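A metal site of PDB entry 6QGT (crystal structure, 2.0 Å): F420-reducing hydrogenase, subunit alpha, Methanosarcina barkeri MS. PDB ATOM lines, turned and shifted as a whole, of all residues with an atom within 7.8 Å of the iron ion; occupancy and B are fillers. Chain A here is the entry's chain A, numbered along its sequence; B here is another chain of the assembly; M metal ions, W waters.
The backbone NH (N) of Glu 44 sits at hydrogen-bond distance from the side-chain amide oxygen (OE1) of Gln 103 of chain B (2.8 Å). A ring nitrogen (ND1) of His 438 sits close to the backbone carbonyl oxygen of Ala 436. O of Cys 435 lies within hydrogen-bond range of ND1 of His 438, at 2.7 Å.
The iron ion is bound by water W2, OE2 of Glu 44, O of Met 399, water W1, water W3 and NE2 of His 438. The iron ion has six donor atoms within binding distance.
Water W3 lies within hydrogen-bond range of the side-chain carboxylate (OE1) of Glu 44 (2.6 Å) and a ring nitrogen (NE2) of His 104 of chain B (2.7 Å). Water W2 lies within hydrogen-bond range of the side-chain carboxylate of Glu 259 (2.5 Å), the side-chain carboxylate of Asp 398 (2.7 Å) and a ring nitrogen (NE2) of His 104 of chain B (3.4 Å).
Three residues have an atom within 4 Å of the iron ion: Glu 44, Met 399 and His 438. The nearest printed residue that does not touch the iron ion is Asp 398 (4.1 Å).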
ATOM      1  N   GLU A  44       2.674  35.499 -12.951  1.00  0.00           N
ATOM      2  CA  GLU A  44       3.549  34.970 -14.001  1.00  0.00           C
ATOM      3  C   GLU A  44       4.348  36.074 -14.700  1.00  0.00           C
ATOM      4  O   GLU A  44       5.540  35.906 -14.985  1.00  0.00           O
ATOM      5  CB  GLU A  44       2.731  34.179 -15.021  1.00  0.00           C
ATOM      6  CG  GLU A  44       2.154  32.926 -14.393  1.00  0.00           C
ATOM      7  CD  GLU A  44       0.880  32.487 -15.056  1.00  0.00           C
ATOM      8  OE1 GLU A  44       0.350  33.278 -15.892  1.00  0.00           O
ATOM      9  OE2 GLU A  44       0.450  31.343 -14.762  1.00  0.00           O
ATOM     10  N   TRP A 257      -0.152  19.279 -22.811  1.00  0.00           N
ATOM     11  CA  TRP A 257      -0.796  20.430 -22.220  1.00  0.00           C
ATOM     12  C   TRP A 257      -0.830  21.569 -23.229  1.00  0.00           C
ATOM     13  O   TRP A 257       0.106  21.748 -24.018  1.00  0.00           O
ATOM     14  CB  TRP A 257      -0.051  20.869 -20.944  1.00  0.00           C
ATOM     15  CG  TRP A 257      -0.234  22.299 -20.696  1.00  0.00           C
ATOM     16  CD1 TRP A 257      -1.377  22.916 -20.298  1.00  0.00           C
ATOM     17  CD2 TRP A 257       0.757  23.325 -20.827  1.00  0.00           C
ATOM     18  NE1 TRP A 257      -1.176  24.260 -20.172  1.00  0.00           N
ATOM     19  CE2 TRP A 257       0.124  24.543 -20.493  1.00  0.00           C
ATOM     20  CE3 TRP A 257       2.113  23.331 -21.176  1.00  0.00           C
ATOM     21  CZ2 TRP A 257       0.792  25.770 -20.516  1.00  0.00           C
ATOM     22  CZ3 TRP A 257       2.781  24.559 -21.199  1.00  0.00           C
ATOM     23  CH2 TRP A 257       2.123  25.751 -20.879  1.00  0.00           C
ATOM     24  N   GLU A 259      -2.713  25.779 -23.052  1.00  0.00           N
ATOM     25  CA  GLU A 259      -3.610  26.705 -22.374  1.00  0.00           C
ATOM     26  C   GLU A 259      -4.147  27.700 -23.387  1.00  0.00           C
ATOM     27  O   GLU A 259      -3.388  28.275 -24.175  1.00  0.00           O
ATOM     28  CB  GLU A 259      -2.902  27.432 -21.212  1.00  0.00           C
ATOM     29  CG  GLU A 259      -3.873  28.212 -20.296  1.00  0.00           C
ATOM     30  CD  GLU A 259      -3.230  28.763 -19.021  1.00  0.00           C
ATOM     31  OE1 GLU A 259      -2.002  28.982 -19.018  1.00  0.00           O
ATOM     32  OE2 GLU A 259      -3.959  29.000 -18.022  1.00  0.00           O
ATOM     33  N   THR A 299      -9.487  33.747 -15.789  1.00  0.00           N
ATOM     34  CA  THR A 299      -8.447  32.740 -15.828  1.00  0.00           C
ATOM     35  C   THR A 299      -8.073  32.418 -17.265  1.00  0.00           C
ATOM     36  O   THR A 299      -8.773  32.772 -18.203  1.00  0.00           O
ATOM     37  CB  THR A 299      -8.901  31.468 -15.100  1.00  0.00           C
ATOM     38  OG1 THR A 299     -10.081  30.947 -15.720  1.00  0.00           O
ATOM     39  CG2 THR A 299      -9.188  31.743 -13.621  1.00  0.00           C
ATOM     40  N   GLY A 300      -6.922  31.750 -17.440  1.00  0.00           N
ATOM     41  CA  GLY A 300      -6.698  30.991 -18.643  1.00  0.00           C
ATOM     42  C   GLY A 300      -7.317  29.615 -18.467  1.00  0.00           C
ATOM     43  O   GLY A 300      -7.732  29.264 -17.371  1.00  0.00           O
ATOM     44  N   VAL A 301      -7.406  28.864 -19.554  1.00  0.00           N
ATOM     45  CA  VAL A 301      -7.985  27.518 -19.530  1.00  0.00           C
ATOM     46  C   VAL A 301      -6.921  26.522 -19.975  1.00  0.00           C
ATOM     47  O   VAL A 301      -6.707  26.313 -21.158  1.00  0.00           O
ATOM     48  CB  VAL A 301      -9.234  27.410 -20.427  1.00  0.00           C
ATOM     49  CG1 VAL A 301      -9.752  25.937 -20.403  1.00  0.00           C
ATOM     50  CG2 VAL A 301     -10.304  28.391 -19.988  1.00  0.00           C
ATOM     51  N   PRO A 302      -6.243  25.886 -19.034  1.00  0.00           N
ATOM     52  CA  PRO A 302      -5.345  24.793 -19.417  1.00  0.00           C
ATOM     53  C   PRO A 302      -6.152  23.582 -19.847  1.00  0.00           C
ATOM     54  O   PRO A 302      -7.243  23.311 -19.320  1.00  0.00           O
ATOM     55  CB  PRO A 302      -4.521  24.516 -18.143  1.00  0.00           C
ATOM     56  CG  PRO A 302      -5.353  25.046 -17.022  1.00  0.00           C
ATOM     57  CD  PRO A 302      -6.182  26.203 -17.605  1.00  0.00           C
ATOM     58  N   ILE A 384       1.086  22.899 -11.303  1.00  0.00           N
ATOM     59  CA  ILE A 384       2.259  22.744 -12.161  1.00  0.00           C
ATOM     60  C   ILE A 384       2.859  24.118 -12.456  1.00  0.00           C
ATOM     61  O   ILE A 384       2.204  24.986 -13.047  1.00  0.00           O
ATOM     62  CB  ILE A 384       1.914  22.000 -13.455  1.00  0.00           C
ATOM     63  CG1 ILE A 384       1.433  20.593 -13.096  1.00  0.00           C
ATOM     64  CG2 ILE A 384       3.137  21.921 -14.376  1.00  0.00           C
ATOM     65  CD1 ILE A 384       0.283  20.147 -13.896  1.00  0.00           C
ATOM     66  N   TYR A 397       8.021  32.168 -16.832  1.00  0.00           N
ATOM     67  CA  TYR A 397       7.329  31.551 -15.712  1.00  0.00           C
ATOM     68  C   TYR A 397       5.886  31.258 -16.093  1.00  0.00           C
ATOM     69  O   TYR A 397       5.255  32.049 -16.797  1.00  0.00           O
ATOM     70  CB  TYR A 397       7.390  32.456 -14.486  1.00  0.00           C
ATOM     71  CG  TYR A 397       7.151  31.704 -13.197  1.00  0.00           C
ATOM     72  CD1 TYR A 397       7.850  30.531 -12.890  1.00  0.00           C
ATOM     73  CD2 TYR A 397       6.221  32.147 -12.283  1.00  0.00           C
ATOM     74  CE1 TYR A 397       7.610  29.847 -11.697  1.00  0.00           C
ATOM     75  CE2 TYR A 397       5.990  31.480 -11.115  1.00  0.00           C
ATOM     76  CZ  TYR A 397       6.681  30.334 -10.821  1.00  0.00           C
ATOM     77  OH  TYR A 397       6.416  29.735  -9.626  1.00  0.00           O
ATOM     78  N   ASP A 398       5.380  30.111 -15.647  1.00  0.00           N
ATOM     79  CA  ASP A 398       4.002  29.766 -15.978  1.00  0.00           C
ATOM     80  C   ASP A 398       3.425  28.908 -14.866  1.00  0.00           C
ATOM     81  O   ASP A 398       4.106  28.017 -14.361  1.00  0.00           O
ATOM     82  CB  ASP A 398       3.917  29.044 -17.334  1.00  0.00           C
ATOM     83  CG  ASP A 398       2.597  29.310 -18.063  1.00  0.00           C
ATOM     84  OD1 ASP A 398       1.765  30.097 -17.561  1.00  0.00           O
ATOM     85  OD2 ASP A 398       2.393  28.741 -19.155  1.00  0.00           O
ATOM     86  N   MET A 399       2.158  29.150 -14.517  1.00  0.00           N
ATOM     87  CA  MET A 399       1.501  28.483 -13.404  1.00  0.00           C
ATOM     88  C   MET A 399       0.160  27.906 -13.865  1.00  0.00           C
ATOM     89  O   MET A 399      -0.736  28.657 -14.295  1.00  0.00           O
ATOM     90  CB  MET A 399       1.311  29.462 -12.227  1.00  0.00           C
ATOM     91  CG  MET A 399       2.566  29.886 -11.529  1.00  0.00           C
ATOM     92  SD  MET A 399       2.266  31.253 -10.370  1.00  0.00           S
ATOM     93  CE  MET A 399       0.962  30.581  -9.286  1.00  0.00           C
ATOM     94  N   LEU A 400       0.024  26.569 -13.779  1.00  0.00           N
ATOM     95  CA  LEU A 400      -1.213  25.855 -14.112  1.00  0.00           C
ATOM     96  C   LEU A 400      -1.755  25.289 -12.797  1.00  0.00           C
ATOM     97  O   LEU A 400      -1.334  24.223 -12.359  1.00  0.00           O
ATOM     98  CB  LEU A 400      -0.937  24.723 -15.127  1.00  0.00           C
ATOM     99  CG  LEU A 400       0.024  25.056 -16.287  1.00  0.00           C
ATOM    100  CD1 LEU A 400       0.387  23.804 -17.120  1.00  0.00           C
ATOM    101  CD2 LEU A 400      -0.564  26.153 -17.168  1.00  0.00           C
ATOM    102  N   VAL A 401      -2.713  25.990 -12.189  1.00  0.00           N
ATOM    103  CA  VAL A 401      -3.103  25.777 -10.792  1.00  0.00           C
ATOM    104  C   VAL A 401      -4.384  24.941 -10.771  1.00  0.00           C
ATOM    105  O   VAL A 401      -5.216  25.079 -11.678  1.00  0.00           O
ATOM    106  CB  VAL A 401      -3.256  27.136 -10.090  1.00  0.00           C
ATOM    107  CG1 VAL A 401      -3.482  27.013  -8.561  1.00  0.00           C
ATOM    108  CG2 VAL A 401      -2.036  27.999 -10.336  1.00  0.00           C
ATOM    109  N   THR A 404      -7.671  26.465 -11.639  1.00  0.00           N
ATOM    110  CA  THR A 404      -7.653  26.883 -13.048  1.00  0.00           C
ATOM    111  C   THR A 404      -8.117  25.729 -13.936  1.00  0.00           C
ATOM    112  O   THR A 404      -8.950  25.918 -14.840  1.00  0.00           O
ATOM    113  CB  THR A 404      -6.244  27.326 -13.462  1.00  0.00           C
ATOM    114  OG1 THR A 404      -5.606  28.058 -12.403  1.00  0.00           O
ATOM    115  CG2 THR A 404      -6.293  28.189 -14.708  1.00  0.00           C
ATOM    116  N   CYS A 435      -6.123  31.185  -6.137  1.00  0.00           N
ATOM    117  CA  CYS A 435      -5.277  30.193  -6.810  1.00  0.00           C
ATOM    118  C   CYS A 435      -5.491  30.160  -8.303  1.00  0.00           C
ATOM    119  O   CYS A 435      -4.535  30.209  -9.094  1.00  0.00           O
ATOM    120  CB  CYS A 435      -5.546  28.808  -6.265  1.00  0.00           C
ATOM    121  SG  CYS A 435      -4.333  28.460  -5.107  1.00  0.00           S
ATOM    122  N   ALA A 436      -6.755  30.013  -8.714  1.00  0.00           N
ATOM    123  CA  ALA A 436      -7.053  29.785 -10.114  1.00  0.00           C
ATOM    124  C   ALA A 436      -6.576  30.923 -10.981  1.00  0.00           C
ATOM    125  O   ALA A 436      -6.232  30.710 -12.144  1.00  0.00           O
ATOM    126  CB  ALA A 436      -8.564  29.620 -10.298  1.00  0.00           C
ATOM    127  N   THR A 437      -6.570  32.137 -10.431  1.00  0.00           N
ATOM    128  CA  THR A 437      -6.367  33.379 -11.184  1.00  0.00           C
ATOM    129  C   THR A 437      -4.918  33.842 -11.122  1.00  0.00           C
ATOM    130  O   THR A 437      -4.373  34.255 -12.144  1.00  0.00           O
ATOM    131  CB  THR A 437      -7.270  34.498 -10.626  1.00  0.00           C
ATOM    132  OG1 THR A 437      -8.640  34.064 -10.589  1.00  0.00           O
ATOM    133  CG2 THR A 437      -7.180  35.751 -11.444  1.00  0.00           C
ATOM    134  N   HIS A 438      -4.306  33.739  -9.943  1.00  0.00           N
ATOM    135  CA  HIS A 438      -2.944  34.187  -9.634  1.00  0.00           C
ATOM    136  C   HIS A 438      -2.544  35.436 -10.431  1.00  0.00           C
ATOM    137  O   HIS A 438      -3.301  36.397 -10.473  1.00  0.00           O
ATOM    138  CB  HIS A 438      -1.929  33.049  -9.866  1.00  0.00           C
ATOM    139  CG  HIS A 438      -2.154  32.231 -11.088  1.00  0.00           C
ATOM    140  ND1 HIS A 438      -3.048  31.168 -11.131  1.00  0.00           N
ATOM    141  CD2 HIS A 438      -1.528  32.230 -12.294  1.00  0.00           C
ATOM    142  CE1 HIS A 438      -2.988  30.594 -12.310  1.00  0.00           C
ATOM    143  NE2 HIS A 438      -2.067  31.209 -13.036  1.00  0.00           N
ATOM    144  N   GLN B 103      -1.129  39.699 -18.047  1.00  0.00           N
ATOM    145  CA  GLN B 103      -1.431  38.280 -17.901  1.00  0.00           C
ATOM    146  C   GLN B 103      -2.878  37.991 -18.265  1.00  0.00           C
ATOM    147  O   GLN B 103      -3.780  38.792 -17.976  1.00  0.00           O
ATOM    148  CB  GLN B 103      -1.154  37.816 -16.461  1.00  0.00           C
ATOM    149  CG  GLN B 103      -1.188  36.318 -16.225  1.00  0.00           C
ATOM    150  CD  GLN B 103      -0.690  35.952 -14.815  1.00  0.00           C
ATOM    151  OE1 GLN B 103       0.455  36.243 -14.452  1.00  0.00           O
ATOM    152  NE2 GLN B 103      -1.568  35.347 -14.008  1.00  0.00           N
ATOM    153  N   HIS B 104      -3.102  36.848 -18.922  1.00  0.00           N
ATOM    154  CA  HIS B 104      -4.473  36.447 -19.205  1.00  0.00           C
ATOM    155  C   HIS B 104      -5.221  36.121 -17.910  1.00  0.00           C
ATOM    156  O   HIS B 104      -4.627  35.696 -16.901  1.00  0.00           O
ATOM    157  CB  HIS B 104      -4.505  35.253 -20.174  1.00  0.00           C
ATOM    158  CG  HIS B 104      -3.789  34.024 -19.678  1.00  0.00           C
ATOM    159  ND1 HIS B 104      -3.234  33.089 -20.553  1.00  0.00           N
ATOM    160  CD2 HIS B 104      -3.596  33.528 -18.428  1.00  0.00           C
ATOM    161  CE1 HIS B 104      -2.709  32.092 -19.855  1.00  0.00           C
ATOM    162  NE2 HIS B 104      -2.917  32.335 -18.562  1.00  0.00           N
HETATM  163 FE    FE M   1      -1.448  30.489 -15.109  1.00  0.00          FE
HETATM  164  O   HOH W   1      -3.435  29.620 -15.632  1.00  0.00           O
HETATM  165  O   HOH W   2      -0.895  30.053 -17.037  1.00  0.00           O
HETATM  166  O   HOH W   3      -2.071  32.462 -16.035  1.00  0.00           O
